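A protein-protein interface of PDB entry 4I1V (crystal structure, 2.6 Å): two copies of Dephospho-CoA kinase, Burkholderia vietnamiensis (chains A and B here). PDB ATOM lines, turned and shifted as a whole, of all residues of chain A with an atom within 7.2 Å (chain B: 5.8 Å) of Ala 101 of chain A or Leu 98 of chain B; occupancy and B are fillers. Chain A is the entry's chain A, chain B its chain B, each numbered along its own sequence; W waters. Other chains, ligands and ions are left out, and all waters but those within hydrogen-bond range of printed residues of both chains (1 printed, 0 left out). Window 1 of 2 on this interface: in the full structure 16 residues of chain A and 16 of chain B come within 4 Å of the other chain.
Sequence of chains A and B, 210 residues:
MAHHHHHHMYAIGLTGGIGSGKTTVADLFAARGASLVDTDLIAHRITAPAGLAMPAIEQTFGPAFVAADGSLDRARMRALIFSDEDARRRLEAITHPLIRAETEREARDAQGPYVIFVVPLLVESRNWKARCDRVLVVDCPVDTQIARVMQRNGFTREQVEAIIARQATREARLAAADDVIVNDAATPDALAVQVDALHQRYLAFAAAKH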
ATOM      1  N   ILE A  42      -6.060 -24.711 -30.198  1.00  0.00           N
ATOM      2  CA  ILE A  42      -6.887 -23.695 -29.590  1.00  0.00           C
ATOM      3  C   ILE A  42      -6.297 -23.224 -28.251  1.00  0.00           C
ATOM      4  O   ILE A  42      -6.205 -22.025 -27.993  1.00  0.00           O
ATOM      5  CB  ILE A  42      -8.317 -24.201 -29.402  1.00  0.00           C
ATOM      6  CG1 ILE A  42      -8.967 -24.367 -30.764  1.00  0.00           C
ATOM      7  CG2 ILE A  42      -9.144 -23.223 -28.585  1.00  0.00           C
ATOM      8  CD1 ILE A  42     -10.259 -25.128 -30.688  1.00  0.00           C
ATOM      9  N   THR A  95      -8.987 -21.537 -18.835  1.00  0.00           N
ATOM     10  CA  THR A  95      -8.706 -21.996 -20.216  1.00  0.00           C
ATOM     11  C   THR A  95      -9.735 -23.009 -20.745  1.00  0.00           C
ATOM     12  O   THR A  95     -10.138 -22.917 -21.892  1.00  0.00           O
ATOM     13  CB  THR A  95      -7.292 -22.608 -20.347  1.00  0.00           C
ATOM     14  OG1 THR A  95      -7.144 -23.656 -19.382  1.00  0.00           O
ATOM     15  CG2 THR A  95      -6.251 -21.563 -20.112  1.00  0.00           C
ATOM     16  N   HIS A  96     -10.165 -23.943 -19.907  1.00  0.00           N
ATOM     17  CA  HIS A  96     -10.999 -25.047 -20.396  1.00  0.00           C
ATOM     18  C   HIS A  96     -12.320 -24.596 -20.962  1.00  0.00           C
ATOM     19  O   HIS A  96     -12.648 -24.944 -22.084  1.00  0.00           O
ATOM     20  CB  HIS A  96     -11.173 -26.138 -19.338  1.00  0.00           C
ATOM     21  CG  HIS A  96      -9.917 -26.915 -19.114  1.00  0.00           C
ATOM     22  ND1 HIS A  96      -9.888 -28.130 -18.464  1.00  0.00           N
ATOM     23  CD2 HIS A  96      -8.637 -26.650 -19.485  1.00  0.00           C
ATOM     24  CE1 HIS A  96      -8.640 -28.569 -18.424  1.00  0.00           C
ATOM     25  NE2 HIS A  96      -7.863 -27.693 -19.043  1.00  0.00           N
ATOM     26  N   PRO A  97     -13.044 -23.759 -20.225  1.00  0.00           N
ATOM     27  CA  PRO A  97     -14.248 -23.210 -20.828  1.00  0.00           C
ATOM     28  C   PRO A  97     -13.985 -22.496 -22.164  1.00  0.00           C
ATOM     29  O   PRO A  97     -14.760 -22.653 -23.094  1.00  0.00           O
ATOM     30  CB  PRO A  97     -14.760 -22.203 -19.770  1.00  0.00           C
ATOM     31  CG  PRO A  97     -14.014 -22.510 -18.526  1.00  0.00           C
ATOM     32  CD  PRO A  97     -12.696 -23.066 -18.979  1.00  0.00           C
ATOM     33  N   LEU A  98     -12.929 -21.707 -22.262  1.00  0.00           N
ATOM     34  CA  LEU A  98     -12.650 -21.016 -23.524  1.00  0.00           C
ATOM     35  C   LEU A  98     -12.289 -22.000 -24.676  1.00  0.00           C
ATOM     36  O   LEU A  98     -12.674 -21.798 -25.824  1.00  0.00           O
ATOM     37  CB  LEU A  98     -11.543 -19.988 -23.336  1.00  0.00           C
ATOM     38  CG  LEU A  98     -11.881 -18.832 -22.392  1.00  0.00           C
ATOM     39  CD1 LEU A  98     -10.640 -18.042 -21.986  1.00  0.00           C
ATOM     40  CD2 LEU A  98     -12.916 -17.902 -23.012  1.00  0.00           C
ATOM     41  N   ILE A  99     -11.591 -23.076 -24.336  1.00  0.00           N
ATOM     42  CA  ILE A  99     -11.270 -24.111 -25.290  1.00  0.00           C
ATOM     43  C   ILE A  99     -12.546 -24.805 -25.766  1.00  0.00           C
ATOM     44  O   ILE A  99     -12.759 -24.962 -26.966  1.00  0.00           O
ATOM     45  CB  ILE A  99     -10.298 -25.144 -24.692  1.00  0.00           C
ATOM     46  CG1 ILE A  99      -8.902 -24.537 -24.579  1.00  0.00           C
ATOM     47  CG2 ILE A  99     -10.244 -26.379 -25.574  1.00  0.00           C
ATOM     48  CD1 ILE A  99      -8.039 -25.226 -23.550  1.00  0.00           C
ATOM     49  N   ARG A 100     -13.355 -25.251 -24.810  1.00  0.00           N
ATOM     50  CA  ARG A 100     -14.686 -25.827 -25.094  1.00  0.00           C
ATOM     51  C   ARG A 100     -15.436 -24.880 -26.036  1.00  0.00           C
ATOM     52  O   ARG A 100     -15.940 -25.320 -27.076  1.00  0.00           O
ATOM     53  CB  ARG A 100     -15.491 -26.162 -23.815  1.00  0.00           C
ATOM     54  N   ALA A 101     -15.420 -23.584 -25.755  1.00  0.00           N
ATOM     55  CA  ALA A 101     -16.195 -22.677 -26.591  1.00  0.00           C
ATOM     56  C   ALA A 101     -15.652 -22.558 -27.997  1.00  0.00           C
ATOM     57  O   ALA A 101     -16.406 -22.673 -28.967  1.00  0.00           O
ATOM     58  CB  ALA A 101     -16.309 -21.299 -25.954  1.00  0.00           C
ATOM     59  N   GLU A 102     -14.360 -22.306 -28.129  1.00  0.00           N
ATOM     60  CA  GLU A 102     -13.765 -22.219 -29.465  1.00  0.00           C
ATOM     61  C   GLU A 102     -13.949 -23.513 -30.310  1.00  0.00           C
ATOM     62  O   GLU A 102     -14.021 -23.476 -31.559  1.00  0.00           O
ATOM     63  CB  GLU A 102     -12.293 -21.882 -29.353  1.00  0.00           C
ATOM     64  CG  GLU A 102     -12.073 -20.450 -28.937  1.00  0.00           C
ATOM     65  CD  GLU A 102     -12.359 -19.459 -30.069  1.00  0.00           C
ATOM     66  OE1 GLU A 102     -11.618 -19.474 -31.079  1.00  0.00           O
ATOM     67  OE2 GLU A 102     -13.321 -18.656 -29.944  1.00  0.00           O
ATOM     68  N   THR A 103     -14.045 -24.640 -29.614  1.00  0.00           N
ATOM     69  CA  THR A 103     -14.240 -25.896 -30.277  1.00  0.00           C
ATOM     70  C   THR A 103     -15.584 -25.896 -30.979  1.00  0.00           C
ATOM     71  O   THR A 103     -15.682 -26.230 -32.173  1.00  0.00           O
ATOM     72  CB  THR A 103     -14.115 -27.070 -29.302  1.00  0.00           C
ATOM     73  OG1 THR A 103     -12.763 -27.148 -28.818  1.00  0.00           O
ATOM     74  CG2 THR A 103     -14.461 -28.368 -30.013  1.00  0.00           C
ATOM     75  N   GLU A 104     -16.625 -25.503 -30.255  1.00  0.00           N
ATOM     76  CA  GLU A 104     -17.951 -25.427 -30.851  1.00  0.00           C
ATOM     77  C   GLU A 104     -18.017 -24.483 -32.047  1.00  0.00           C
ATOM     78  O   GLU A 104     -18.681 -24.774 -33.067  1.00  0.00           O
ATOM     79  CB  GLU A 104     -18.969 -25.012 -29.815  1.00  0.00           C
ATOM     80  CG  GLU A 104     -19.085 -25.946 -28.620  1.00  0.00           C
ATOM     81  CD  GLU A 104     -19.456 -27.361 -28.968  1.00  0.00           C
ATOM     82  OE1 GLU A 104     -19.892 -27.615 -30.109  1.00  0.00           O
ATOM     83  OE2 GLU A 104     -19.344 -28.215 -28.063  1.00  0.00           O
ATOM     84  N   ARG A 105     -17.296 -23.385 -31.928  1.00  0.00           N
ATOM     85  CA  ARG A 105     -17.287 -22.365 -32.947  1.00  0.00           C
ATOM     86  C   ARG A 105     -16.540 -22.839 -34.208  1.00  0.00           C
ATOM     87  O   ARG A 105     -16.939 -22.509 -35.324  1.00  0.00           O
ATOM     88  CB  ARG A 105     -16.686 -21.078 -32.365  1.00  0.00           C
ATOM     89  CG  ARG A 105     -16.807 -19.869 -33.283  1.00  0.00           C
ATOM     90  CD  ARG A 105     -15.989 -18.641 -32.827  1.00  0.00           C
ATOM     91  NE  ARG A 105     -15.670 -18.685 -31.403  1.00  0.00           N
ATOM     92  CZ  ARG A 105     -16.475 -18.288 -30.401  1.00  0.00           C
ATOM     93  NH1 ARG A 105     -17.690 -17.779 -30.631  1.00  0.00           N
ATOM     94  NH2 ARG A 105     -16.054 -18.405 -29.145  1.00  0.00           N
ATOM     95  N   GLU A 106     -15.454 -23.599 -34.034  1.00  0.00           N
ATOM     96  CA  GLU A 106     -14.696 -24.119 -35.178  1.00  0.00           C
ATOM     97  C   GLU A 106     -15.472 -25.270 -35.814  1.00  0.00           C
ATOM     98  O   GLU A 106     -15.428 -25.460 -37.036  1.00  0.00           O
ATOM     99  CB  GLU A 106     -13.298 -24.581 -34.768  1.00  0.00           C
ATOM    100  CG  GLU A 106     -12.328 -23.482 -34.319  1.00  0.00           C
ATOM    101  CD  GLU A 106     -11.547 -22.848 -35.463  1.00  0.00           C
ATOM    102  OE1 GLU A 106     -11.954 -23.008 -36.636  1.00  0.00           O
ATOM    103  OE2 GLU A 106     -10.519 -22.171 -35.202  1.00  0.00           O
ATOM    104  N   ALA A 107     -16.190 -26.017 -34.984  1.00  0.00           N
ATOM    105  CA  ALA A 107     -16.997 -27.121 -35.456  1.00  0.00           C
ATOM    106  C   ALA A 107     -18.199 -26.624 -36.263  1.00  0.00           C
ATOM    107  O   ALA A 107     -18.547 -27.193 -37.290  1.00  0.00           O
ATOM    108  CB  ALA A 107     -17.460 -27.962 -34.283  1.00  0.00           C
ATOM    109  N   ILE B  42     -27.194 -13.780 -23.566  1.00  0.00           N
ATOM    110  CA  ILE B  42     -26.276 -14.684 -24.198  1.00  0.00           C
ATOM    111  C   ILE B  42     -26.821 -16.117 -24.044  1.00  0.00           C
ATOM    112  O   ILE B  42     -26.874 -16.854 -25.002  1.00  0.00           O
ATOM    113  CB  ILE B  42     -24.846 -14.538 -23.612  1.00  0.00           C
ATOM    114  CG1 ILE B  42     -24.231 -13.183 -23.971  1.00  0.00           C
ATOM    115  CG2 ILE B  42     -23.924 -15.629 -24.123  1.00  0.00           C
ATOM    116  CD1 ILE B  42     -22.955 -12.868 -23.213  1.00  0.00           C
ATOM    117  N   ILE B  46     -27.413 -18.357 -27.400  1.00  0.00           N
ATOM    118  CA  ILE B  46     -26.685 -19.585 -27.708  1.00  0.00           C
ATOM    119  C   ILE B  46     -27.594 -20.821 -27.756  1.00  0.00           C
ATOM    120  O   ILE B  46     -27.150 -21.891 -28.174  1.00  0.00           O
ATOM    121  CB  ILE B  46     -25.516 -19.883 -26.741  1.00  0.00           C
ATOM    122  CG1 ILE B  46     -26.051 -20.255 -25.363  1.00  0.00           C
ATOM    123  CG2 ILE B  46     -24.524 -18.734 -26.682  1.00  0.00           C
ATOM    124  CD1 ILE B  46     -24.968 -20.734 -24.432  1.00  0.00           C
ATOM    125  N   LEU B  52     -24.937 -21.321 -30.847  1.00  0.00           N
ATOM    126  CA  LEU B  52     -23.659 -21.978 -30.594  1.00  0.00           C
ATOM    127  C   LEU B  52     -23.699 -23.210 -29.680  1.00  0.00           C
ATOM    128  O   LEU B  52     -22.778 -24.021 -29.720  1.00  0.00           O
ATOM    129  CB  LEU B  52     -22.710 -20.943 -29.985  1.00  0.00           C
ATOM    130  CG  LEU B  52     -21.221 -21.263 -29.890  1.00  0.00           C
ATOM    131  CD1 LEU B  52     -20.598 -21.290 -31.279  1.00  0.00           C
ATOM    132  CD2 LEU B  52     -20.552 -20.215 -29.008  1.00  0.00           C
ATOM    133  N   ALA B  53     -24.744 -23.350 -28.871  1.00  0.00           N
ATOM    134  CA  ALA B  53     -24.866 -24.452 -27.910  1.00  0.00           C
ATOM    135  C   ALA B  53     -25.694 -25.625 -28.405  1.00  0.00           C
ATOM    136  O   ALA B  53     -25.707 -26.690 -27.779  1.00  0.00           O
ATOM    137  CB  ALA B  53     -25.475 -23.943 -26.615  1.00  0.00           C
ATOM    138  N   ILE B  94     -22.630 -27.570 -20.610  1.00  0.00           N
ATOM    139  CA  ILE B  94     -22.523 -27.108 -21.983  1.00  0.00           C
ATOM    140  C   ILE B  94     -22.645 -25.598 -22.065  1.00  0.00           C
ATOM    141  O   ILE B  94     -21.852 -24.946 -22.737  1.00  0.00           O
ATOM    142  CB  ILE B  94     -23.596 -27.735 -22.871  1.00  0.00           C
ATOM    143  CG1 ILE B  94     -23.282 -29.225 -23.083  1.00  0.00           C
ATOM    144  CG2 ILE B  94     -23.685 -27.011 -24.213  1.00  0.00           C
ATOM    145  CD1 ILE B  94     -24.474 -30.011 -23.572  1.00  0.00           C
ATOM    146  N   THR B  95     -23.632 -25.042 -21.377  1.00  0.00           N
ATOM    147  CA  THR B  95     -23.974 -23.650 -21.572  1.00  0.00           C
ATOM    148  C   THR B  95     -23.004 -22.719 -20.862  1.00  0.00           C
ATOM    149  O   THR B  95     -22.641 -21.674 -21.419  1.00  0.00           O
ATOM    150  CB  THR B  95     -25.422 -23.340 -21.142  1.00  0.00           C
ATOM    151  OG1 THR B  95     -25.621 -23.750 -19.793  1.00  0.00           O
ATOM    152  CG2 THR B  95     -26.404 -24.066 -22.019  1.00  0.00           C
ATOM    153  N   HIS B  96     -22.585 -23.067 -19.647  1.00  0.00           N
ATOM    154  CA  HIS B  96     -21.822 -22.099 -18.823  1.00  0.00           C
ATOM    155  C   HIS B  96     -20.492 -21.701 -19.440  1.00  0.00           C
ATOM    156  O   HIS B  96     -20.227 -20.512 -19.598  1.00  0.00           O
ATOM    157  CB  HIS B  96     -21.695 -22.561 -17.368  1.00  0.00           C
ATOM    158  CG  HIS B  96     -22.999 -22.486 -16.627  1.00  0.00           C
ATOM    159  ND1 HIS B  96     -23.087 -22.542 -15.252  1.00  0.00           N
ATOM    160  CD2 HIS B  96     -24.269 -22.314 -17.081  1.00  0.00           C
ATOM    161  CE1 HIS B  96     -24.356 -22.427 -14.892  1.00  0.00           C
ATOM    162  NE2 HIS B  96     -25.093 -22.288 -15.984  1.00  0.00           N
ATOM    163  N   PRO B  97     -19.696 -22.677 -19.879  1.00  0.00           N
ATOM    164  CA  PRO B  97     -18.459 -22.324 -20.576  1.00  0.00           C
ATOM    165  C   PRO B  97     -18.712 -21.456 -21.815  1.00  0.00           C
ATOM    166  O   PRO B  97     -17.988 -20.500 -22.050  1.00  0.00           O
ATOM    167  CB  PRO B  97     -17.878 -23.676 -20.978  1.00  0.00           C
ATOM    168  CG  PRO B  97     -18.615 -24.692 -20.163  1.00  0.00           C
ATOM    169  CD  PRO B  97     -19.969 -24.117 -19.920  1.00  0.00           C
ATOM    170  N   LEU B  98     -19.757 -21.740 -22.582  1.00  0.00           N
ATOM    171  CA  LEU B  98     -20.045 -20.888 -23.756  1.00  0.00           C
ATOM    172  C   LEU B  98     -20.451 -19.466 -23.366  1.00  0.00           C
ATOM    173  O   LEU B  98     -20.104 -18.496 -24.039  1.00  0.00           O
ATOM    174  CB  LEU B  98     -21.120 -21.528 -24.649  1.00  0.00           C
ATOM    175  CG  LEU B  98     -20.686 -22.867 -25.246  1.00  0.00           C
ATOM    176  CD1 LEU B  98     -21.873 -23.615 -25.815  1.00  0.00           C
ATOM    177  CD2 LEU B  98     -19.623 -22.674 -26.322  1.00  0.00           C
ATOM    178  N   ILE B  99     -21.229 -19.361 -22.294  1.00  0.00           N
ATOM    179  CA  ILE B  99     -21.673 -18.069 -21.812  1.00  0.00           C
ATOM    180  C   ILE B  99     -20.461 -17.272 -21.322  1.00  0.00           C
ATOM    181  O   ILE B  99     -20.258 -16.137 -21.697  1.00  0.00           O
ATOM    182  CB  ILE B  99     -22.680 -18.218 -20.667  1.00  0.00           C
ATOM    183  CG1 ILE B  99     -24.035 -18.659 -21.198  1.00  0.00           C
ATOM    184  CG2 ILE B  99     -22.810 -16.906 -19.922  1.00  0.00           C
ATOM    185  CD1 ILE B  99     -24.890 -19.323 -20.142  1.00  0.00           C
ATOM    186  N   ARG B 100     -19.664 -17.919 -20.490  1.00  0.00           N
ATOM    187  CA  ARG B 100     -18.359 -17.435 -20.109  1.00  0.00           C
ATOM    188  C   ARG B 100     -17.585 -16.905 -21.302  1.00  0.00           C
ATOM    189  O   ARG B 100     -17.071 -15.786 -21.276  1.00  0.00           O
ATOM    190  CB  ARG B 100     -17.586 -18.591 -19.471  1.00  0.00           C
ATOM    191  CG  ARG B 100     -16.638 -18.206 -18.362  1.00  0.00           C
ATOM    192  CD  ARG B 100     -17.323 -17.507 -17.186  1.00  0.00           C
ATOM    193  NE  ARG B 100     -16.291 -16.958 -16.302  1.00  0.00           N
ATOM    194  CZ  ARG B 100     -15.553 -15.878 -16.562  1.00  0.00           C
ATOM    195  NH1 ARG B 100     -15.736 -15.154 -17.671  1.00  0.00           N
ATOM    196  NH2 ARG B 100     -14.623 -15.514 -15.692  1.00  0.00           N
ATOM    197  N   ALA B 101     -17.496 -17.695 -22.362  1.00  0.00           N
ATOM    198  CA  ALA B 101     -16.686 -17.276 -23.495  1.00  0.00           C
ATOM    199  C   ALA B 101     -17.270 -16.060 -24.202  1.00  0.00           C
ATOM    200  O   ALA B 101     -16.553 -15.086 -24.430  1.00  0.00           O
ATOM    201  CB  ALA B 101     -16.478 -18.406 -24.464  1.00  0.00           C
ATOM    202  N   GLU B 102     -18.556 -16.100 -24.536  1.00  0.00           N
ATOM    203  CA  GLU B 102     -19.206 -14.961 -25.207  1.00  0.00           C
ATOM    204  C   GLU B 102     -19.105 -13.662 -24.371  1.00  0.00           C
ATOM    205  O   GLU B 102     -19.077 -12.533 -24.894  1.00  0.00           O
ATOM    206  CB  GLU B 102     -20.661 -15.305 -25.521  1.00  0.00           C
ATOM    207  CG  GLU B 102     -20.812 -16.369 -26.610  1.00  0.00           C
ATOM    208  CD  GLU B 102     -20.472 -15.842 -27.992  1.00  0.00           C
ATOM    209  OE1 GLU B 102     -21.247 -14.979 -28.494  1.00  0.00           O
ATOM    210  OE2 GLU B 102     -19.429 -16.280 -28.560  1.00  0.00           O
ATOM    211  N   THR B 103     -19.013 -13.840 -23.062  1.00  0.00           N
ATOM    212  CA  THR B 103     -18.878 -12.725 -22.177  1.00  0.00           C
ATOM    213  C   THR B 103     -17.538 -12.027 -22.366  1.00  0.00           C
ATOM    214  O   THR B 103     -17.498 -10.811 -22.551  1.00  0.00           O
ATOM    215  CB  THR B 103     -19.050 -13.156 -20.715  1.00  0.00           C
ATOM    216  OG1 THR B 103     -20.398 -13.616 -20.530  1.00  0.00           O
ATOM    217  CG2 THR B 103     -18.791 -11.982 -19.795  1.00  0.00           C
HETATM  218  O   HOH W   1     -22.585 -26.740 -29.508  1.00  0.00           O
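Among the printed residues, merely in contact across the chains: Ala 101 of chain A with Ala 101 of chain B, Ala 101 of chain A with Leu 98 of chain B, Pro 97 of chain A with Pro 97 of chain B, Leu 98 of chain A with Ala 101 of chain B, Arg 105 of chain A with Leu 52 of chain B and Glu 104 of chain A with Leu 52 of chain B.
Pro 97 of chain B touches its own counterpart, Pro 97 of chain A.
Leu 98 of chain A touches Ala 101 of chain B, and with the chains exchanged Ala 101 of chain A touches Leu 98 of chain B.
Ala 101 of chain B touches its own counterpart, Ala 101 of chain A.
Positions printed for both chains: 42, 95, 96, 97, 98, 99, 100, 101, 102 and 103.
Of the 7 pairs that touch across the chains among the printed residues, 4 have their exchanged pair printed and touching as well.
NH1 of Arg 105 of chain A is in salt-bridge range of OE2 of Glu 102 of chain B, 3.1 Å away.
Water W1 bridges O of Leu 52 of chain B (2.7 Å) and OE1 of Glu 104 of chain A (2.9 Å).
Of the 14 printed residues of chain A, 5 touch a printed residue of chain B.
Hydrophobic or aromatic side chains of chain A within 4 Å of the printed part of chain B: Pro 97, Leu 98 and Ala 101.
Of the 14 printed residues of chain B, 5 touch a printed residue of chain A.
Printed residues of chain B that touch a printed residue of chain A: Leu 52, Pro 97, Leu 98, Ala 101 and Glu 102.
Ile 42 of chain A touches none of the printed residues of chain B.
Printed residues of chain B within 4 Å of Pro 97 of chain A: Pro 97 (3.7 Å).
Printed residues of chain B within 4 Å of Leu 98 of chain A: Ala 101 (3.9 Å).
Of the printed residues of chain B, Ala 101 of chain A touches Leu 98 and Ala 101.
Of the printed residues of chain B, Arg 105 of chain A touches Leu 52 (3.9 Å) and Glu 102 (3.1 Å).
Printed residues of chain A within 4 Å of Pro 97 of chain B: Pro 97 (3.7 Å).
Printed residues of chain A within 4 Å of Ala 101 of chain B: Leu 98 and Ala 101.
NE of Arg 105 of chain A lies within salt-bridge range of OE2 of Glu 102 of chain A, 2.8 Å away.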
